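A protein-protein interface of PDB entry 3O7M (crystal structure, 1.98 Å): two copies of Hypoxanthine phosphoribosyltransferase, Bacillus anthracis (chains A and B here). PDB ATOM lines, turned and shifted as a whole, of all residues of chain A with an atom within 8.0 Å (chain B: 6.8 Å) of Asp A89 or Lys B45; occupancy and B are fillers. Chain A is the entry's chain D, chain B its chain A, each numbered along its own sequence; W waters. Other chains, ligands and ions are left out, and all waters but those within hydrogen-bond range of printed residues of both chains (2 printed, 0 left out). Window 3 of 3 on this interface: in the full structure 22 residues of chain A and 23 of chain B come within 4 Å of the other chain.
Asp A89 touches one residue of chain B.
Printed residues of chain A within 4 Å of Lys B45: Asp A65 (2.9 Å), Phe A66 (3.97 Å) and Asp A89 (3.0 Å).
No residue of chain A comes within 4 Å of Gly B46.
Of the printed residues of chain A, Phe B48 touches Ile A64 (3.7 Å) and Phe A66 (3.8 Å).
Of the printed residues of chain A, Arg B167 touches Ile A64.
Of the printed residues of chain B, Thr A63 touches Glu B164 (3.9 Å).
Printed residues of chain B within 4 Å of Asp A65: Lys B45.
Glu B101 touches none of the printed residues of chain A.
Ile A67 touches none of the printed residues of chain B.
The nearest residue of chain B that does not touch Asp A89 is Leu B85 (6.0 Å).
The nearest printed residue of chain B that does not touch Thr A63 is Arg B167 (6.0 Å).
Water W2 lies within hydrogen-bond range of the side-chain carboxylate (OE1) of Glu B164, the side-chain amino group (NZ) of Lys B45 and the backbone carbonyl oxygen (O) of Ile A64.
Water W1 lies within hydrogen-bond range of OE1 of Glu B164 (2.6 Å), N of Ile A64 (2.9 Å) and NE of Arg B167 (3.0 Å).
Among the printed residues, pairs that only touch across the chains: Ile A64 with Arg B167 (3.5 Å), Ile A64 with Phe B48 (3.7 Å), Phe A66 with Phe B48 (3.8 Å), Thr A63 with Glu B164 (3.9 Å), Ile A64 with Glu B164 (3.96 Å) and Phe A66 with Lys B45 (3.97 Å).
Hydrophobic or aromatic side chains of chain A within 4 Å of the printed part of chain B: Ile A64 and Phe A66.
Among the printed residues, 8 pairs touch across the chains.
Among the printed residues, Asp or Glu carboxylates within 4 Å of a Lys or Arg side-chain nitrogen of the other chain: Asp A65 with Lys B45 and Asp A89 with Lys B45.
Position printed for both chains: 67.
NH1 of Arg B167 lies within hydrogen-bond range of O of Gly B159, at 2.8 Å.
OE1 of Glu B164 lies within salt-bridge range of NH2 of Arg B167 (3.1 Å).
The side-chain carboxylate (OD2) of Asp A65 lies within hydrogen-bond range of the backbone NH (N) of Asp A89, at 2.7 Å.
The backbone NH (N) of Val A90 lies within hydrogen-bond range of the side-chain carboxylate (OD2) of Asp A65, 3.0 Å away.
The side-chain amino group (NZ) of Lys A86 is in salt-bridge range of the side-chain carboxylate (OD2) of Asp A89 (3.0 Å).
The side-chain carboxylate of Asp A65 lies within salt-bridge range of the side-chain amino group of Lys B45 (2.9 Å).
The side-chain amino group of Lys B45 is in salt-bridge range of the side-chain carboxylate of Asp A89 (3.0 Å).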
ATOM      1  N   ILE A  41     -22.604 -13.160  -7.274  1.00  0.00           N
ATOM      2  CA  ILE A  41     -23.240 -13.069  -5.974  1.00  0.00           C
ATOM      3  C   ILE A  41     -23.704 -14.477  -5.580  1.00  0.00           C
ATOM      4  O   ILE A  41     -24.560 -15.082  -6.242  1.00  0.00           O
ATOM      5  CB  ILE A  41     -24.447 -12.146  -6.000  1.00  0.00           C
ATOM      6  CG1 ILE A  41     -24.052 -10.740  -6.412  1.00  0.00           C
ATOM      7  CG2 ILE A  41     -25.100 -12.118  -4.605  1.00  0.00           C
ATOM      8  CD1 ILE A  41     -25.223  -9.879  -6.652  1.00  0.00           C
ATOM      9  N   THR A  63     -15.637  -9.960  -9.121  1.00  0.00           N
ATOM     10  CA  THR A  63     -15.910  -9.424  -7.791  1.00  0.00           C
ATOM     11  C   THR A  63     -16.904 -10.407  -7.209  1.00  0.00           C
ATOM     12  O   THR A  63     -17.782 -10.880  -7.939  1.00  0.00           O
ATOM     13  CB  THR A  63     -16.567  -8.044  -7.882  1.00  0.00           C
ATOM     14  OG1 THR A  63     -15.604  -7.121  -8.364  1.00  0.00           O
ATOM     15  CG2 THR A  63     -17.081  -7.585  -6.530  1.00  0.00           C
ATOM     16  N   ILE A  64     -16.794 -10.744  -5.932  1.00  0.00           N
ATOM     17  CA  ILE A  64     -17.770 -11.652  -5.348  1.00  0.00           C
ATOM     18  C   ILE A  64     -18.412 -11.077  -4.081  1.00  0.00           C
ATOM     19  O   ILE A  64     -17.813 -10.297  -3.351  1.00  0.00           O
ATOM     20  CB  ILE A  64     -17.235 -13.123  -5.239  1.00  0.00           C
ATOM     21  CG1 ILE A  64     -18.168 -14.039  -4.420  1.00  0.00           C
ATOM     22  CG2 ILE A  64     -15.837 -13.162  -4.699  1.00  0.00           C
ATOM     23  CD1 ILE A  64     -18.160 -15.522  -4.944  1.00  0.00           C
ATOM     24  N   ASP A  65     -19.675 -11.430  -3.873  1.00  0.00           N
ATOM     25  CA  ASP A  65     -20.371 -11.006  -2.687  1.00  0.00           C
ATOM     26  C   ASP A  65     -21.405 -12.065  -2.395  1.00  0.00           C
ATOM     27  O   ASP A  65     -21.562 -13.034  -3.168  1.00  0.00           O
ATOM     28  CB  ASP A  65     -20.971  -9.610  -2.867  1.00  0.00           C
ATOM     29  CG  ASP A  65     -21.196  -8.881  -1.532  1.00  0.00           C
ATOM     30  OD1 ASP A  65     -21.024  -9.482  -0.452  1.00  0.00           O
ATOM     31  OD2 ASP A  65     -21.570  -7.699  -1.581  1.00  0.00           O
ATOM     32  N   PHE A  66     -22.080 -11.901  -1.263  1.00  0.00           N
ATOM     33  CA  PHE A  66     -23.026 -12.876  -0.786  1.00  0.00           C
ATOM     34  C   PHE A  66     -24.346 -12.224  -0.399  1.00  0.00           C
ATOM     35  O   PHE A  66     -24.412 -11.052  -0.019  1.00  0.00           O
ATOM     36  CB  PHE A  66     -22.458 -13.588   0.460  1.00  0.00           C
ATOM     37  CG  PHE A  66     -21.174 -14.297   0.209  1.00  0.00           C
ATOM     38  CD1 PHE A  66     -19.971 -13.638   0.382  1.00  0.00           C
ATOM     39  CD2 PHE A  66     -21.164 -15.590  -0.272  1.00  0.00           C
ATOM     40  CE1 PHE A  66     -18.782 -14.287   0.118  1.00  0.00           C
ATOM     41  CE2 PHE A  66     -19.971 -16.240  -0.549  1.00  0.00           C
ATOM     42  CZ  PHE A  66     -18.784 -15.589  -0.356  1.00  0.00           C
ATOM     43  N   ILE A  67     -25.409 -12.999  -0.513  1.00  0.00           N
ATOM     44  CA  ILE A  67     -26.717 -12.539  -0.075  1.00  0.00           C
ATOM     45  C   ILE A  67     -27.333 -13.649   0.723  1.00  0.00           C
ATOM     46  O   ILE A  67     -27.068 -14.841   0.460  1.00  0.00           O
ATOM     47  CB  ILE A  67     -27.570 -12.138  -1.289  1.00  0.00           C
ATOM     48  CG1 ILE A  67     -28.747 -11.287  -0.849  1.00  0.00           C
ATOM     49  CG2 ILE A  67     -27.967 -13.383  -2.100  1.00  0.00           C
ATOM     50  CD1 ILE A  67     -29.250 -10.293  -1.938  1.00  0.00           C
ATOM     51  N   LYS A  86     -29.374 -10.500   4.656  1.00  0.00           N
ATOM     52  CA  LYS A  86     -28.105  -9.839   4.390  1.00  0.00           C
ATOM     53  C   LYS A  86     -28.089  -9.441   2.927  1.00  0.00           C
ATOM     54  O   LYS A  86     -28.131 -10.290   2.039  1.00  0.00           O
ATOM     55  CB  LYS A  86     -26.921 -10.770   4.660  1.00  0.00           C
ATOM     56  CG  LYS A  86     -25.540 -10.157   4.261  1.00  0.00           C
ATOM     57  CD  LYS A  86     -25.169  -8.978   5.192  1.00  0.00           C
ATOM     58  CE  LYS A  86     -23.794  -8.326   4.864  1.00  0.00           C
ATOM     59  NZ  LYS A  86     -23.788  -7.350   3.687  1.00  0.00           N
ATOM     60  N   ASP A  87     -28.064  -8.149   2.694  1.00  0.00           N
ATOM     61  CA  ASP A  87     -28.029  -7.585   1.364  1.00  0.00           C
ATOM     62  C   ASP A  87     -26.572  -7.490   0.911  1.00  0.00           C
ATOM     63  O   ASP A  87     -25.649  -7.645   1.705  1.00  0.00           O
ATOM     64  CB  ASP A  87     -28.647  -6.200   1.437  1.00  0.00           C
ATOM     65  CG  ASP A  87     -29.181  -5.687   0.100  1.00  0.00           C
ATOM     66  OD1 ASP A  87     -29.033  -6.319  -0.987  1.00  0.00           O
ATOM     67  OD2 ASP A  87     -29.802  -4.609   0.151  1.00  0.00           O
ATOM     68  N   ILE A  88     -26.365  -7.242  -0.373  1.00  0.00           N
ATOM     69  CA  ILE A  88     -25.008  -7.100  -0.888  1.00  0.00           C
ATOM     70  C   ILE A  88     -24.367  -5.773  -0.481  1.00  0.00           C
ATOM     71  O   ILE A  88     -25.055  -4.774  -0.269  1.00  0.00           O
ATOM     72  CB  ILE A  88     -24.984  -7.211  -2.430  1.00  0.00           C
ATOM     73  CG1 ILE A  88     -25.812  -6.121  -3.107  1.00  0.00           C
ATOM     74  CG2 ILE A  88     -25.476  -8.604  -2.837  1.00  0.00           C
ATOM     75  CD1 ILE A  88     -25.736  -6.113  -4.654  1.00  0.00           C
ATOM     76  N   ASP A  89     -23.040  -5.781  -0.391  1.00  0.00           N
ATOM     77  CA  ASP A  89     -22.253  -4.598  -0.148  1.00  0.00           C
ATOM     78  C   ASP A  89     -21.690  -3.987  -1.426  1.00  0.00           C
ATOM     79  O   ASP A  89     -21.484  -2.766  -1.508  1.00  0.00           O
ATOM     80  CB  ASP A  89     -21.049  -4.965   0.713  1.00  0.00           C
ATOM     81  CG  ASP A  89     -21.447  -5.548   2.030  1.00  0.00           C
ATOM     82  OD1 ASP A  89     -20.908  -6.616   2.386  1.00  0.00           O
ATOM     83  OD2 ASP A  89     -22.323  -4.944   2.666  1.00  0.00           O
ATOM     84  N   VAL A  90     -21.408  -4.825  -2.424  1.00  0.00           N
ATOM     85  CA  VAL A  90     -20.763  -4.322  -3.617  1.00  0.00           C
ATOM     86  C   VAL A  90     -21.713  -3.601  -4.561  1.00  0.00           C
ATOM     87  O   VAL A  90     -22.910  -3.814  -4.554  1.00  0.00           O
ATOM     88  CB  VAL A  90     -20.014  -5.443  -4.401  1.00  0.00           C
ATOM     89  CG1 VAL A  90     -18.924  -6.103  -3.457  1.00  0.00           C
ATOM     90  CG2 VAL A  90     -21.003  -6.465  -4.996  1.00  0.00           C
ATOM     91  N   ASN A  91     -21.120  -2.783  -5.409  1.00  0.00           N
ATOM     92  CA  ASN A  91     -21.844  -2.061  -6.458  1.00  0.00           C
ATOM     93  C   ASN A  91     -22.075  -2.990  -7.661  1.00  0.00           C
ATOM     94  O   ASN A  91     -21.135  -3.568  -8.172  1.00  0.00           O
ATOM     95  CB  ASN A  91     -20.966  -0.906  -6.911  1.00  0.00           C
ATOM     96  CG  ASN A  91     -21.586  -0.090  -8.039  1.00  0.00           C
ATOM     97  OD1 ASN A  91     -22.792  -0.073  -8.225  1.00  0.00           O
ATOM     98  ND2 ASN A  91     -20.743   0.580  -8.793  1.00  0.00           N
ATOM     99  N   ILE A  92     -23.321  -3.148  -8.090  1.00  0.00           N
ATOM    100  CA  ILE A  92     -23.646  -3.914  -9.287  1.00  0.00           C
ATOM    101  C   ILE A  92     -24.297  -3.010 -10.355  1.00  0.00           C
ATOM    102  O   ILE A  92     -24.652  -3.470 -11.434  1.00  0.00           O
ATOM    103  CB  ILE A  92     -24.568  -5.119  -8.994  1.00  0.00           C
ATOM    104  CG1 ILE A  92     -25.909  -4.699  -8.416  1.00  0.00           C
ATOM    105  CG2 ILE A  92     -23.871  -6.086  -8.021  1.00  0.00           C
ATOM    106  CD1 ILE A  92     -26.928  -5.867  -8.384  1.00  0.00           C
ATOM    107  N   PHE A 117     -32.413  -7.386  -7.242  1.00  0.00           N
ATOM    108  CA  PHE A 117     -31.196  -6.919  -7.905  1.00  0.00           C
ATOM    109  C   PHE A 117     -31.515  -6.039  -9.082  1.00  0.00           C
ATOM    110  O   PHE A 117     -30.746  -5.130  -9.383  1.00  0.00           O
ATOM    111  CB  PHE A 117     -30.277  -8.059  -8.332  1.00  0.00           C
ATOM    112  CG  PHE A 117     -29.680  -8.818  -7.202  1.00  0.00           C
ATOM    113  CD1 PHE A 117     -28.980  -8.154  -6.197  1.00  0.00           C
ATOM    114  CD2 PHE A 117     -29.815 -10.179  -7.133  1.00  0.00           C
ATOM    115  CE1 PHE A 117     -28.425  -8.835  -5.168  1.00  0.00           C
ATOM    116  CE2 PHE A 117     -29.237 -10.886  -6.096  1.00  0.00           C
ATOM    117  CZ  PHE A 117     -28.542 -10.200  -5.103  1.00  0.00           C
ATOM    118  N   HIS A 120     -31.227  -2.415  -8.579  1.00  0.00           N
ATOM    119  CA  HIS A 120     -29.902  -1.794  -8.603  1.00  0.00           C
ATOM    120  C   HIS A 120     -29.413  -1.380 -10.000  1.00  0.00           C
ATOM    121  O   HIS A 120     -28.328  -0.841 -10.138  1.00  0.00           O
ATOM    122  CB  HIS A 120     -28.872  -2.777  -8.034  1.00  0.00           C
ATOM    123  CG  HIS A 120     -28.951  -2.947  -6.548  1.00  0.00           C
ATOM    124  ND1 HIS A 120     -27.852  -2.824  -5.729  1.00  0.00           N
ATOM    125  CD2 HIS A 120     -29.990  -3.253  -5.734  1.00  0.00           C
ATOM    126  CE1 HIS A 120     -28.204  -3.038  -4.477  1.00  0.00           C
ATOM    127  NE2 HIS A 120     -29.504  -3.275  -4.447  1.00  0.00           N
ATOM    128  N   VAL B  43     -15.142 -17.169   8.658  1.00  0.00           N
ATOM    129  CA  VAL B  43     -15.246 -15.737   8.776  1.00  0.00           C
ATOM    130  C   VAL B  43     -15.341 -15.147   7.366  1.00  0.00           C
ATOM    131  O   VAL B  43     -14.401 -15.212   6.564  1.00  0.00           O
ATOM    132  CB  VAL B  43     -14.046 -15.092   9.517  1.00  0.00           C
ATOM    133  CG1 VAL B  43     -14.260 -13.567   9.668  1.00  0.00           C
ATOM    134  CG2 VAL B  43     -13.825 -15.746  10.914  1.00  0.00           C
ATOM    135  N   LEU B  44     -16.481 -14.562   7.044  1.00  0.00           N
ATOM    136  CA  LEU B  44     -16.632 -13.987   5.703  1.00  0.00           C
ATOM    137  C   LEU B  44     -15.791 -12.714   5.556  1.00  0.00           C
ATOM    138  O   LEU B  44     -15.445 -12.087   6.542  1.00  0.00           O
ATOM    139  CB  LEU B  44     -18.104 -13.686   5.441  1.00  0.00           C
ATOM    140  CG  LEU B  44     -19.031 -14.877   5.288  1.00  0.00           C
ATOM    141  CD1 LEU B  44     -20.500 -14.364   5.361  1.00  0.00           C
ATOM    142  CD2 LEU B  44     -18.716 -15.617   3.981  1.00  0.00           C
ATOM    143  N   LYS B  45     -15.417 -12.343   4.334  1.00  0.00           N
ATOM    144  CA  LYS B  45     -15.740 -13.084   3.118  1.00  0.00           C
ATOM    145  C   LYS B  45     -14.600 -13.956   2.645  1.00  0.00           C
ATOM    146  O   LYS B  45     -14.813 -15.034   2.129  1.00  0.00           O
ATOM    147  CB  LYS B  45     -16.023 -12.111   1.961  1.00  0.00           C
ATOM    148  CG  LYS B  45     -17.229 -11.223   2.214  1.00  0.00           C
ATOM    149  CD  LYS B  45     -17.416 -10.111   1.198  1.00  0.00           C
ATOM    150  CE  LYS B  45     -18.527  -9.192   1.659  1.00  0.00           C
ATOM    151  NZ  LYS B  45     -18.823  -8.017   0.814  1.00  0.00           N
ATOM    152  N   GLY B  46     -13.379 -13.470   2.818  1.00  0.00           N
ATOM    153  CA  GLY B  46     -12.202 -14.086   2.215  1.00  0.00           C
ATOM    154  C   GLY B  46     -11.855 -15.534   2.510  1.00  0.00           C
ATOM    155  O   GLY B  46     -11.109 -16.154   1.770  1.00  0.00           O
ATOM    156  N   SER B  47     -12.373 -16.097   3.586  1.00  0.00           N
ATOM    157  CA  SER B  47     -12.009 -17.426   3.923  1.00  0.00           C
ATOM    158  C   SER B  47     -12.845 -18.488   3.220  1.00  0.00           C
ATOM    159  O   SER B  47     -12.595 -19.668   3.418  1.00  0.00           O
ATOM    160  CB  SER B  47     -12.220 -17.599   5.429  1.00  0.00           C
ATOM    161  OG  SER B  47     -13.606 -17.663   5.704  1.00  0.00           O
ATOM    162  N   PHE B  48     -13.846 -18.087   2.434  1.00  0.00           N
ATOM    163  CA  PHE B  48     -14.808 -19.069   1.925  1.00  0.00           C
ATOM    164  C   PHE B  48     -14.200 -20.103   1.010  1.00  0.00           C
ATOM    165  O   PHE B  48     -14.674 -21.229   0.991  1.00  0.00           O
ATOM    166  CB  PHE B  48     -16.061 -18.432   1.298  1.00  0.00           C
ATOM    167  CG  PHE B  48     -15.915 -18.043  -0.133  1.00  0.00           C
ATOM    168  CD1 PHE B  48     -16.475 -18.828  -1.142  1.00  0.00           C
ATOM    169  CD2 PHE B  48     -15.243 -16.876  -0.489  1.00  0.00           C
ATOM    170  CE1 PHE B  48     -16.351 -18.443  -2.468  1.00  0.00           C
ATOM    171  CE2 PHE B  48     -15.140 -16.484  -1.812  1.00  0.00           C
ATOM    172  CZ  PHE B  48     -15.681 -17.278  -2.798  1.00  0.00           C
ATOM    173  N   VAL B  49     -13.163 -19.739   0.267  1.00  0.00           N
ATOM    174  CA  VAL B  49     -12.527 -20.698  -0.665  1.00  0.00           C
ATOM    175  C   VAL B  49     -11.738 -21.744   0.122  1.00  0.00           C
ATOM    176  O   VAL B  49     -11.892 -22.955  -0.070  1.00  0.00           O
ATOM    177  CB  VAL B  49     -11.670 -19.963  -1.679  1.00  0.00           C
ATOM    178  CG1 VAL B  49     -10.908 -20.941  -2.571  1.00  0.00           C
ATOM    179  CG2 VAL B  49     -12.560 -19.024  -2.552  1.00  0.00           C
ATOM    180  N   ILE B  67     -19.789 -16.260   9.909  1.00  0.00           N
ATOM    181  CA  ILE B  67     -19.847 -15.110  10.752  1.00  0.00           C
ATOM    182  C   ILE B  67     -19.296 -13.938   9.997  1.00  0.00           C
ATOM    183  O   ILE B  67     -18.382 -14.071   9.153  1.00  0.00           O
ATOM    184  CB  ILE B  67     -19.045 -15.329  12.059  1.00  0.00           C
ATOM    185  CG1 ILE B  67     -19.304 -14.207  13.061  1.00  0.00           C
ATOM    186  CG2 ILE B  67     -17.558 -15.467  11.780  1.00  0.00           C
ATOM    187  CD1 ILE B  67     -20.166 -14.579  14.151  1.00  0.00           C
ATOM    188  N   SER B  68     -19.877 -12.767  10.254  1.00  0.00           N
ATOM    189  CA  SER B  68     -19.416 -11.522   9.642  1.00  0.00           C
ATOM    190  C   SER B  68     -19.281 -10.439  10.711  1.00  0.00           C
ATOM    191  O   SER B  68     -20.189 -10.232  11.536  1.00  0.00           O
ATOM    192  CB  SER B  68     -20.377 -11.030   8.559  1.00  0.00           C
ATOM    193  OG  SER B  68     -20.352 -11.874   7.435  1.00  0.00           O
ATOM    194  N   LEU B  85     -21.956  -8.225  12.223  1.00  0.00           N
ATOM    195  CA  LEU B  85     -22.901  -7.984  11.132  1.00  0.00           C
ATOM    196  C   LEU B  85     -23.866  -9.140  10.909  1.00  0.00           C
ATOM    197  O   LEU B  85     -25.026  -8.926  10.572  1.00  0.00           O
ATOM    198  CB  LEU B  85     -22.164  -7.724   9.828  1.00  0.00           C
ATOM    199  CG  LEU B  85     -21.168  -6.573   9.818  1.00  0.00           C
ATOM    200  CD1 LEU B  85     -20.570  -6.393   8.383  1.00  0.00           C
ATOM    201  CD2 LEU B  85     -21.865  -5.326  10.259  1.00  0.00           C
ATOM    202  N   GLU B 101     -10.206 -18.693   8.997  1.00  0.00           N
ATOM    203  CA  GLU B 101      -9.851 -17.372   8.468  1.00  0.00           C
ATOM    204  C   GLU B 101      -8.877 -17.460   7.301  1.00  0.00           C
ATOM    205  O   GLU B 101      -8.143 -18.453   7.150  1.00  0.00           O
ATOM    206  CB  GLU B 101      -9.208 -16.509   9.572  1.00  0.00           C
ATOM    207  CG  GLU B 101     -10.103 -15.450  10.141  1.00  0.00           C
ATOM    208  CD  GLU B 101     -10.386 -14.296   9.148  1.00  0.00           C
ATOM    209  OE1 GLU B 101     -10.462 -13.163   9.617  1.00  0.00           O
ATOM    210  OE2 GLU B 101     -10.526 -14.496   7.909  1.00  0.00           O
ATOM    211  N   ASP B 102      -8.847 -16.411   6.480  1.00  0.00           N
ATOM    212  CA  ASP B 102      -7.894 -16.354   5.378  1.00  0.00           C
ATOM    213  C   ASP B 102      -6.509 -15.875   5.904  1.00  0.00           C
ATOM    214  O   ASP B 102      -5.464 -16.474   5.639  1.00  0.00           O
ATOM    215  CB  ASP B 102      -8.435 -15.457   4.236  1.00  0.00           C
ATOM    216  CG  ASP B 102      -8.922 -14.065   4.710  1.00  0.00           C
ATOM    217  OD1 ASP B 102      -9.155 -13.801   5.928  1.00  0.00           O
ATOM    218  OD2 ASP B 102      -9.088 -13.195   3.827  1.00  0.00           O
ATOM    219  N   GLY B 159      -9.570 -16.561  -2.590  1.00  0.00           N
ATOM    220  CA  GLY B 159     -10.564 -15.908  -1.709  1.00  0.00           C
ATOM    221  C   GLY B 159     -10.206 -14.518  -1.219  1.00  0.00           C
ATOM    222  O   GLY B 159     -11.105 -13.737  -0.877  1.00  0.00           O
ATOM    223  N   GLU B 164     -11.528  -5.688  -3.546  1.00  0.00           N
ATOM    224  CA  GLU B 164     -12.544  -6.610  -4.066  1.00  0.00           C
ATOM    225  C   GLU B 164     -12.099  -7.449  -5.286  1.00  0.00           C
ATOM    226  O   GLU B 164     -12.833  -8.352  -5.675  1.00  0.00           O
ATOM    227  CB  GLU B 164     -13.888  -5.911  -4.358  1.00  0.00           C
ATOM    228  CG  GLU B 164     -14.603  -5.350  -3.100  1.00  0.00           C
ATOM    229  CD  GLU B 164     -14.936  -6.391  -2.028  1.00  0.00           C
ATOM    230  OE1 GLU B 164     -15.105  -7.603  -2.315  1.00  0.00           O
ATOM    231  OE2 GLU B 164     -15.026  -5.993  -0.855  1.00  0.00           O
ATOM    232  N   ARG B 167      -9.927 -12.331  -5.930  1.00  0.00           N
ATOM    233  CA  ARG B 167     -10.356 -13.470  -5.105  1.00  0.00           C
ATOM    234  C   ARG B 167     -10.462 -14.751  -5.923  1.00  0.00           C
ATOM    235  O   ARG B 167     -10.367 -15.837  -5.372  1.00  0.00           O
ATOM    236  CB  ARG B 167     -11.708 -13.252  -4.463  1.00  0.00           C
ATOM    237  CG  ARG B 167     -11.828 -12.046  -3.567  1.00  0.00           C
ATOM    238  CD  ARG B 167     -13.131 -12.132  -2.821  1.00  0.00           C
ATOM    239  NE  ARG B 167     -13.499 -10.927  -2.084  1.00  0.00           N
ATOM    240  CZ  ARG B 167     -13.228 -10.663  -0.814  1.00  0.00           C
ATOM    241  NH1 ARG B 167     -12.454 -11.448  -0.093  1.00  0.00           N
ATOM    242  NH2 ARG B 167     -13.682  -9.532  -0.293  1.00  0.00           N
HETATM  243  O   HOH W   1     -14.815  -9.380  -4.252  1.00  0.00           O
HETATM  244  O   HOH W   2     -17.406  -8.456  -1.410  1.00  0.00           O
